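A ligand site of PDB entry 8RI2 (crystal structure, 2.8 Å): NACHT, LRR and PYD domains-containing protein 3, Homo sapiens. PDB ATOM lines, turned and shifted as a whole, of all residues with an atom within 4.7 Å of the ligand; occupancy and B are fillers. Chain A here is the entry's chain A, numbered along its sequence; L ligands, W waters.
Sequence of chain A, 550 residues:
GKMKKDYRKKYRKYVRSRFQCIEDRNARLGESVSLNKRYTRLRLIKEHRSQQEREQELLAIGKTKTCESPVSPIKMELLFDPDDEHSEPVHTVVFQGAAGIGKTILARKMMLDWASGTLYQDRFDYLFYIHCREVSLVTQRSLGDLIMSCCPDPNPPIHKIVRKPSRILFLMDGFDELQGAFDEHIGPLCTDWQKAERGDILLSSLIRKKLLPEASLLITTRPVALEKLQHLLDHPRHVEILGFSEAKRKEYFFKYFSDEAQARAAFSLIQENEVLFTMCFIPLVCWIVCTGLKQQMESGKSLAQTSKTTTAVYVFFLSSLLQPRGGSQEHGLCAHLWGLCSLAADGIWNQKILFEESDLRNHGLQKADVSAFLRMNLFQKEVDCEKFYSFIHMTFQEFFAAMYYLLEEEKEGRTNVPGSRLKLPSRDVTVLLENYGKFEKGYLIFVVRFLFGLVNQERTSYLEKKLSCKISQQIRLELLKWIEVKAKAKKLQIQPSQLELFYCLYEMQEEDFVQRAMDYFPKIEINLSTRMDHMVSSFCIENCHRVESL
A sulfur (S1) of the ligand sits close to the backbone carbonyl oxygen (O) of Ala 99. Residues that only touch the ligand: Ala 98, Val 224, Ile 282, Leu 284, Tyr 314, Thr 395, Phe 446, Gln 495, Ser 497, Leu 499, Tyr 503 and Met 532. Hydrophobic or aromatic side chains within 4 Å of the ligand: Ala 98, Ala 99, Val 224, Ile 282, Leu 284, Tyr 314, Phe 446, Leu 499, Tyr 503 and Met 532. Of the 23 residues printed, 16 come within 4 Å of the ligand. Along chain A the residues within 4 Å of the ligand span positions 98 to 532. The nearest printed residue that does not touch the ligand is Met 279 (4.01 Å).
The backbone NH (N) of Leu 499 sits close to the side-chain hydroxyl (OG) of Ser 497 (3.5 Å). OD1 of Asp 533 is in hydrogen-bond range of OH of Tyr 503 (2.6 Å). OG1 of Thr 395 is in hydrogen-bond range of OH of Tyr 314. N of Glu 500 lies within hydrogen-bond range of OG of Ser 497 (3.1 Å). The side-chain carboxylate (OE2) of Glu 507 sits at hydrogen-bond distance from the side-chain hydroxyl (OG1) of Thr 310. The side-chain carboxylate (OE1) of Glu 500 is in salt-bridge range of the guanidinium group (NH2) of Arg 449 (2.8 Å). The side-chain amide oxygen (OE1) of Gln 495 lies within hydrogen-bond range of the backbone NH (N) of Ser 497, at 3.5 Å. N of Leu 284 lies within hydrogen-bond range of O of Gly 100 (3.1 Å).
Water W1 lies within hydrogen-bond range of OD1 of Asp 533 (2.7 Å) and N4 of the ligand (2.9 Å).
O3 of the ligand sits at hydrogen-bond distance from NH2 of Arg 449 (2.7 Å). The side-chain carboxylate of Glu 500 is in salt-bridge range of a nitrogen (N5) of the ligand (2.7 Å). The side-chain hydroxyl (OG1) of Thr 310 lies within hydrogen-bond range of an oxygen (O2) of the ligand.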
ATOM      1  N   ALA A  98     -16.871   9.299  -9.143  1.00  0.00           N
ATOM      2  CA  ALA A  98     -17.224  10.590  -9.698  1.00  0.00           C
ATOM      3  C   ALA A  98     -18.275  11.348  -8.825  1.00  0.00           C
ATOM      4  O   ALA A  98     -18.828  10.752  -7.898  1.00  0.00           O
ATOM      5  CB  ALA A  98     -17.707  10.419 -11.124  1.00  0.00           C
ATOM      6  N   ALA A  99     -18.508  12.662  -9.096  1.00  0.00           N
ATOM      7  CA  ALA A  99     -19.481  13.479  -8.356  1.00  0.00           C
ATOM      8  C   ALA A  99     -20.844  12.801  -8.301  1.00  0.00           C
ATOM      9  O   ALA A  99     -21.280  12.267  -9.299  1.00  0.00           O
ATOM     10  CB  ALA A  99     -19.588  14.840  -9.012  1.00  0.00           C
ATOM     11  N   GLY A 100     -21.441  12.721  -7.135  1.00  0.00           N
ATOM     12  CA  GLY A 100     -22.747  12.098  -6.962  1.00  0.00           C
ATOM     13  C   GLY A 100     -22.830  10.587  -7.090  1.00  0.00           C
ATOM     14  O   GLY A 100     -23.931  10.040  -7.032  1.00  0.00           O
ATOM     15  N   VAL A 224     -10.523  13.005 -10.795  1.00  0.00           N
ATOM     16  CA  VAL A 224      -9.753  14.203 -11.119  1.00  0.00           C
ATOM     17  C   VAL A 224      -8.629  14.481 -10.094  1.00  0.00           C
ATOM     18  O   VAL A 224      -7.494  14.758 -10.487  1.00  0.00           O
ATOM     19  CB  VAL A 224     -10.655  15.445 -11.354  1.00  0.00           C
ATOM     20  CG1 VAL A 224     -11.327  15.387 -12.725  1.00  0.00           C
ATOM     21  CG2 VAL A 224     -11.695  15.595 -10.249  1.00  0.00           C
ATOM     22  N   MET A 279     -27.887   7.882 -17.840  1.00  0.00           N
ATOM     23  CA  MET A 279     -27.414   8.785 -16.790  1.00  0.00           C
ATOM     24  C   MET A 279     -27.793   8.329 -15.400  1.00  0.00           C
ATOM     25  O   MET A 279     -27.154   8.749 -14.456  1.00  0.00           O
ATOM     26  CB  MET A 279     -28.001  10.175 -16.971  1.00  0.00           C
ATOM     27  CG  MET A 279     -27.513  10.875 -18.186  1.00  0.00           C
ATOM     28  SD  MET A 279     -28.111  12.574 -18.198  1.00  0.00           S
ATOM     29  CE  MET A 279     -26.973  13.285 -19.337  1.00  0.00           C
ATOM     30  N   PHE A 281     -27.180   5.829 -13.840  1.00  0.00           N
ATOM     31  CA  PHE A 281     -26.189   4.985 -13.183  1.00  0.00           C
ATOM     32  C   PHE A 281     -25.639   5.788 -11.955  1.00  0.00           C
ATOM     33  O   PHE A 281     -25.330   5.199 -10.937  1.00  0.00           O
ATOM     34  CB  PHE A 281     -25.068   4.568 -14.146  1.00  0.00           C
ATOM     35  CG  PHE A 281     -23.985   5.595 -14.406  1.00  0.00           C
ATOM     36  CD1 PHE A 281     -22.780   5.551 -13.728  1.00  0.00           C
ATOM     37  CD2 PHE A 281     -24.157   6.588 -15.363  1.00  0.00           C
ATOM     38  CE1 PHE A 281     -21.793   6.485 -13.985  1.00  0.00           C
ATOM     39  CE2 PHE A 281     -23.148   7.500 -15.630  1.00  0.00           C
ATOM     40  CZ  PHE A 281     -21.981   7.449 -14.938  1.00  0.00           C
ATOM     41  N   ILE A 282     -25.553   7.128 -12.058  1.00  0.00           N
ATOM     42  CA  ILE A 282     -25.134   7.985 -10.960  1.00  0.00           C
ATOM     43  C   ILE A 282     -26.310   8.040 -10.000  1.00  0.00           C
ATOM     44  O   ILE A 282     -27.380   8.500 -10.391  1.00  0.00           O
ATOM     45  CB  ILE A 282     -24.856   9.405 -11.496  1.00  0.00           C
ATOM     46  CG1 ILE A 282     -23.811   9.390 -12.589  1.00  0.00           C
ATOM     47  CG2 ILE A 282     -24.485  10.352 -10.401  1.00  0.00           C
ATOM     48  CD1 ILE A 282     -24.257  10.121 -13.796  1.00  0.00           C
ATOM     49  N   LEU A 284     -26.939  10.120  -7.598  1.00  0.00           N
ATOM     50  CA  LEU A 284     -27.433  11.494  -7.474  1.00  0.00           C
ATOM     51  C   LEU A 284     -28.417  11.817  -8.621  1.00  0.00           C
ATOM     52  O   LEU A 284     -29.446  12.439  -8.368  1.00  0.00           O
ATOM     53  CB  LEU A 284     -26.267  12.487  -7.433  1.00  0.00           C
ATOM     54  CG  LEU A 284     -26.622  13.979  -7.559  1.00  0.00           C
ATOM     55  CD1 LEU A 284     -27.357  14.476  -6.339  1.00  0.00           C
ATOM     56  CD2 LEU A 284     -25.402  14.795  -7.814  1.00  0.00           C
ATOM     57  N   VAL A 285     -28.142  11.337  -9.866  1.00  0.00           N
ATOM     58  CA  VAL A 285     -29.063  11.513 -10.987  1.00  0.00           C
ATOM     59  C   VAL A 285     -30.391  10.813 -10.686  1.00  0.00           C
ATOM     60  O   VAL A 285     -31.443  11.400 -10.891  1.00  0.00           O
ATOM     61  CB  VAL A 285     -28.474  11.110 -12.353  1.00  0.00           C
ATOM     62  CG1 VAL A 285     -29.537  11.111 -13.438  1.00  0.00           C
ATOM     63  CG2 VAL A 285     -27.322  12.032 -12.743  1.00  0.00           C
ATOM     64  N   THR A 310     -27.127  16.806 -19.004  1.00  0.00           N
ATOM     65  CA  THR A 310     -27.084  17.048 -17.552  1.00  0.00           C
ATOM     66  C   THR A 310     -27.698  18.445 -17.297  1.00  0.00           C
ATOM     67  O   THR A 310     -28.434  18.625 -16.332  1.00  0.00           O
ATOM     68  CB  THR A 310     -25.637  17.033 -17.022  1.00  0.00           C
ATOM     69  OG1 THR A 310     -24.943  15.900 -17.520  1.00  0.00           O
ATOM     70  CG2 THR A 310     -25.576  16.997 -15.509  1.00  0.00           C
ATOM     71  N   TYR A 314     -30.743  19.339 -14.729  1.00  0.00           N
ATOM     72  CA  TYR A 314     -30.561  20.337 -13.690  1.00  0.00           C
ATOM     73  C   TYR A 314     -31.511  21.493 -13.822  1.00  0.00           C
ATOM     74  O   TYR A 314     -31.977  22.007 -12.821  1.00  0.00           O
ATOM     75  CB  TYR A 314     -29.119  20.801 -13.615  1.00  0.00           C
ATOM     76  CG  TYR A 314     -28.304  19.938 -12.688  1.00  0.00           C
ATOM     77  CD1 TYR A 314     -28.146  18.572 -12.925  1.00  0.00           C
ATOM     78  CD2 TYR A 314     -27.750  20.459 -11.535  1.00  0.00           C
ATOM     79  CE1 TYR A 314     -27.434  17.767 -12.043  1.00  0.00           C
ATOM     80  CE2 TYR A 314     -27.016  19.661 -10.659  1.00  0.00           C
ATOM     81  CZ  TYR A 314     -26.884  18.313 -10.907  1.00  0.00           C
ATOM     82  OH  TYR A 314     -26.216  17.523 -10.007  1.00  0.00           O
ATOM     83  N   THR A 395     -22.232  19.495  -7.226  1.00  0.00           N
ATOM     84  CA  THR A 395     -22.672  19.699  -8.597  1.00  0.00           C
ATOM     85  C   THR A 395     -23.735  20.798  -8.722  1.00  0.00           C
ATOM     86  O   THR A 395     -23.875  21.376  -9.791  1.00  0.00           O
ATOM     87  CB  THR A 395     -23.167  18.400  -9.202  1.00  0.00           C
ATOM     88  OG1 THR A 395     -24.177  17.865  -8.355  1.00  0.00           O
ATOM     89  CG2 THR A 395     -22.059  17.394  -9.393  1.00  0.00           C
ATOM     90  N   ILE A 445     -14.827  21.181 -13.419  1.00  0.00           N
ATOM     91  CA  ILE A 445     -15.351  20.257 -14.408  1.00  0.00           C
ATOM     92  C   ILE A 445     -16.836  20.518 -14.710  1.00  0.00           C
ATOM     93  O   ILE A 445     -17.212  20.675 -15.866  1.00  0.00           O
ATOM     94  CB  ILE A 445     -15.113  18.770 -14.001  1.00  0.00           C
ATOM     95  CG1 ILE A 445     -13.649  18.499 -13.591  1.00  0.00           C
ATOM     96  CG2 ILE A 445     -15.588  17.812 -15.071  1.00  0.00           C
ATOM     97  CD1 ILE A 445     -12.655  18.716 -14.674  1.00  0.00           C
ATOM     98  N   PHE A 446     -17.657  20.582 -13.662  1.00  0.00           N
ATOM     99  CA  PHE A 446     -19.082  20.809 -13.829  1.00  0.00           C
ATOM    100  C   PHE A 446     -19.444  22.273 -14.042  1.00  0.00           C
ATOM    101  O   PHE A 446     -20.499  22.544 -14.593  1.00  0.00           O
ATOM    102  CB  PHE A 446     -19.883  20.201 -12.681  1.00  0.00           C
ATOM    103  CG  PHE A 446     -19.910  18.697 -12.790  1.00  0.00           C
ATOM    104  CD1 PHE A 446     -20.788  18.055 -13.637  1.00  0.00           C
ATOM    105  CD2 PHE A 446     -18.997  17.928 -12.080  1.00  0.00           C
ATOM    106  CE1 PHE A 446     -20.788  16.680 -13.752  1.00  0.00           C
ATOM    107  CE2 PHE A 446     -18.997  16.553 -12.196  1.00  0.00           C
ATOM    108  CZ  PHE A 446     -19.897  15.931 -13.022  1.00  0.00           C
ATOM    109  N   ARG A 449     -18.770  22.417 -17.851  1.00  0.00           N
ATOM    110  CA  ARG A 449     -19.770  21.568 -18.481  1.00  0.00           C
ATOM    111  C   ARG A 449     -21.172  22.215 -18.507  1.00  0.00           C
ATOM    112  O   ARG A 449     -21.811  22.221 -19.548  1.00  0.00           O
ATOM    113  CB  ARG A 449     -19.843  20.245 -17.720  1.00  0.00           C
ATOM    114  CG  ARG A 449     -19.833  19.048 -18.603  1.00  0.00           C
ATOM    115  CD  ARG A 449     -19.978  17.856 -17.728  1.00  0.00           C
ATOM    116  NE  ARG A 449     -18.743  17.081 -17.723  1.00  0.00           N
ATOM    117  CZ  ARG A 449     -18.671  15.820 -17.312  1.00  0.00           C
ATOM    118  NH1 ARG A 449     -19.752  15.191 -16.856  1.00  0.00           N
ATOM    119  NH2 ARG A 449     -17.505  15.172 -17.346  1.00  0.00           N
ATOM    120  N   GLN A 495      -6.265  17.721 -17.892  1.00  0.00           N
ATOM    121  CA  GLN A 495      -7.651  18.167 -18.101  1.00  0.00           C
ATOM    122  C   GLN A 495      -7.720  19.539 -18.831  1.00  0.00           C
ATOM    123  O   GLN A 495      -6.956  20.450 -18.518  1.00  0.00           O
ATOM    124  CB  GLN A 495      -8.431  18.172 -16.761  1.00  0.00           C
ATOM    125  CG  GLN A 495      -9.857  17.620 -16.868  1.00  0.00           C
ATOM    126  CD  GLN A 495      -9.958  16.160 -17.295  1.00  0.00           C
ATOM    127  OE1 GLN A 495     -10.828  15.772 -18.070  1.00  0.00           O
ATOM    128  NE2 GLN A 495      -9.103  15.299 -16.781  1.00  0.00           N
ATOM    129  N   SER A 497      -9.381  16.384 -21.197  1.00  0.00           N
ATOM    130  CA  SER A 497      -9.013  15.349 -22.130  1.00  0.00           C
ATOM    131  C   SER A 497      -9.928  15.524 -23.372  1.00  0.00           C
ATOM    132  O   SER A 497     -10.838  16.365 -23.356  1.00  0.00           O
ATOM    133  CB  SER A 497      -9.212  13.978 -21.495  1.00  0.00           C
ATOM    134  OG  SER A 497     -10.589  13.664 -21.333  1.00  0.00           O
ATOM    135  N   LEU A 499     -12.106  13.287 -24.465  1.00  0.00           N
ATOM    136  CA  LEU A 499     -13.403  12.790 -24.016  1.00  0.00           C
ATOM    137  C   LEU A 499     -14.111  13.828 -23.166  1.00  0.00           C
ATOM    138  O   LEU A 499     -15.305  14.014 -23.320  1.00  0.00           O
ATOM    139  CB  LEU A 499     -13.235  11.487 -23.221  1.00  0.00           C
ATOM    140  CG  LEU A 499     -14.508  10.749 -22.807  1.00  0.00           C
ATOM    141  CD1 LEU A 499     -15.375  10.411 -24.012  1.00  0.00           C
ATOM    142  CD2 LEU A 499     -14.176   9.495 -22.034  1.00  0.00           C
ATOM    143  N   GLU A 500     -13.373  14.561 -22.333  1.00  0.00           N
ATOM    144  CA  GLU A 500     -13.960  15.613 -21.527  1.00  0.00           C
ATOM    145  C   GLU A 500     -14.491  16.741 -22.407  1.00  0.00           C
ATOM    146  O   GLU A 500     -15.606  17.186 -22.173  1.00  0.00           O
ATOM    147  CB  GLU A 500     -12.978  16.108 -20.456  1.00  0.00           C
ATOM    148  CG  GLU A 500     -13.531  17.211 -19.587  1.00  0.00           C
ATOM    149  CD  GLU A 500     -14.800  16.855 -18.836  1.00  0.00           C
ATOM    150  OE1 GLU A 500     -14.899  15.707 -18.336  1.00  0.00           O
ATOM    151  OE2 GLU A 500     -15.709  17.719 -18.744  1.00  0.00           O
ATOM    152  N   TYR A 503     -17.770  15.719 -23.703  1.00  0.00           N
ATOM    153  CA  TYR A 503     -18.835  15.919 -22.715  1.00  0.00           C
ATOM    154  C   TYR A 503     -19.341  17.357 -22.747  1.00  0.00           C
ATOM    155  O   TYR A 503     -20.543  17.587 -22.609  1.00  0.00           O
ATOM    156  CB  TYR A 503     -18.350  15.553 -21.303  1.00  0.00           C
ATOM    157  CG  TYR A 503     -18.545  14.095 -20.967  1.00  0.00           C
ATOM    158  CD1 TYR A 503     -17.655  13.139 -21.402  1.00  0.00           C
ATOM    159  CD2 TYR A 503     -19.640  13.677 -20.224  1.00  0.00           C
ATOM    160  CE1 TYR A 503     -17.827  11.794 -21.107  1.00  0.00           C
ATOM    161  CE2 TYR A 503     -19.840  12.335 -19.932  1.00  0.00           C
ATOM    162  CZ  TYR A 503     -18.920  11.392 -20.371  1.00  0.00           C
ATOM    163  OH  TYR A 503     -19.109  10.072 -20.094  1.00  0.00           O
ATOM    164  N   GLU A 507     -23.092  18.814 -23.833  1.00  0.00           N
ATOM    165  CA  GLU A 507     -23.938  19.767 -23.096  1.00  0.00           C
ATOM    166  C   GLU A 507     -24.413  20.881 -24.042  1.00  0.00           C
ATOM    167  O   GLU A 507     -25.568  21.313 -23.969  1.00  0.00           O
ATOM    168  CB  GLU A 507     -23.195  20.368 -21.906  1.00  0.00           C
ATOM    169  CG  GLU A 507     -22.801  19.338 -20.866  1.00  0.00           C
ATOM    170  CD  GLU A 507     -23.950  18.578 -20.245  1.00  0.00           C
ATOM    171  OE1 GLU A 507     -25.001  19.206 -19.974  1.00  0.00           O
ATOM    172  OE2 GLU A 507     -23.790  17.360 -19.999  1.00  0.00           O
ATOM    173  N   MET A 532     -22.053   5.872 -20.759  1.00  0.00           N
ATOM    174  CA  MET A 532     -22.197   7.318 -20.834  1.00  0.00           C
ATOM    175  C   MET A 532     -21.110   7.845 -21.795  1.00  0.00           C
ATOM    176  O   MET A 532     -21.387   8.739 -22.587  1.00  0.00           O
ATOM    177  CB  MET A 532     -22.013   7.919 -19.440  1.00  0.00           C
ATOM    178  CG  MET A 532     -22.419   9.344 -19.358  1.00  0.00           C
ATOM    179  SD  MET A 532     -24.195   9.565 -19.591  1.00  0.00           S
ATOM    180  CE  MET A 532     -24.177  10.838 -20.847  1.00  0.00           C
ATOM    181  N   ASP A 533     -19.882   7.285 -21.737  1.00  0.00           N
ATOM    182  CA  ASP A 533     -18.782   7.649 -22.630  1.00  0.00           C
ATOM    183  C   ASP A 533     -19.166   7.313 -24.059  1.00  0.00           C
ATOM    184  O   ASP A 533     -18.876   8.104 -24.958  1.00  0.00           O
ATOM    185  CB  ASP A 533     -17.493   6.889 -22.269  1.00  0.00           C
ATOM    186  CG  ASP A 533     -16.849   7.256 -20.965  1.00  0.00           C
ATOM    187  OD1 ASP A 533     -17.261   8.255 -20.360  1.00  0.00           O
ATOM    188  OD2 ASP A 533     -15.938   6.525 -20.525  1.00  0.00           O
HETATM  189  C1  LIG L   1     -20.848  11.821 -13.856  1.00  0.00           C
HETATM  190  C2  LIG L   1     -20.940  12.043 -12.485  1.00  0.00           C
HETATM  191  C3  LIG L   1     -21.982  12.961 -12.310  1.00  0.00           C
HETATM  192  C4  LIG L   1     -21.963  12.445 -15.931  1.00  0.00           C
HETATM  193  C5  LIG L   1     -23.113  13.186 -16.716  1.00  0.00           C
HETATM  194  C6  LIG L   1     -19.066  10.593 -16.833  1.00  0.00           C
HETATM  195  C7  LIG L   1     -17.933  11.591 -16.938  1.00  0.00           C
HETATM  196  C8  LIG L   1     -22.938  13.002 -18.223  1.00  0.00           C
HETATM  197  C9  LIG L   1     -24.476  12.699 -16.253  1.00  0.00           C
HETATM  198  C10 LIG L   1     -15.677  12.058 -17.799  1.00  0.00           C
HETATM  199  C11 LIG L   1     -14.908  12.629 -16.610  1.00  0.00           C
HETATM  200  C12 LIG L   1     -12.883  12.939 -18.017  1.00  0.00           C
HETATM  201  C13 LIG L   1     -13.638  12.407 -19.228  1.00  0.00           C
HETATM  202  C14 LIG L   1     -14.735  11.425 -18.810  1.00  0.00           C
HETATM  203  C15 LIG L   1     -13.103  14.172 -15.890  1.00  0.00           C
HETATM  204  C16 LIG L   1     -22.514  13.291 -13.530  1.00  0.00           C
HETATM  205  N1  LIG L   1     -21.831  12.593 -14.513  1.00  0.00           N
HETATM  206  C17 LIG L   1     -23.563  14.234 -13.464  1.00  0.00           C
HETATM  207  C18 LIG L   1     -23.797  14.590 -12.183  1.00  0.00           C
HETATM  208  S1  LIG L   1     -22.783  13.820 -11.042  1.00  0.00           S
HETATM  209  C19 LIG L   1     -19.909  11.028 -14.596  1.00  0.00           C
HETATM  210  N2  LIG L   1     -20.106  11.084 -15.959  1.00  0.00           N
HETATM  211  N3  LIG L   1     -21.172  11.693 -16.591  1.00  0.00           N
HETATM  212  O1  LIG L   1     -18.938  10.451 -14.114  1.00  0.00           O
HETATM  213  O2  LIG L   1     -23.008  14.590 -16.429  1.00  0.00           O
HETATM  214  N4  LIG L   1     -16.799  11.166 -17.513  1.00  0.00           N
HETATM  215  O3  LIG L   1     -18.047  12.720 -16.457  1.00  0.00           O
HETATM  216 CL1  LIG L   1     -24.937  15.748 -11.645  1.00  0.00          CL
HETATM  217  N5  LIG L   1     -13.832  13.595 -17.055  1.00  0.00           N
HETATM  218  O   HOH W   1     -16.653   8.265 -17.770  1.00  0.00           O
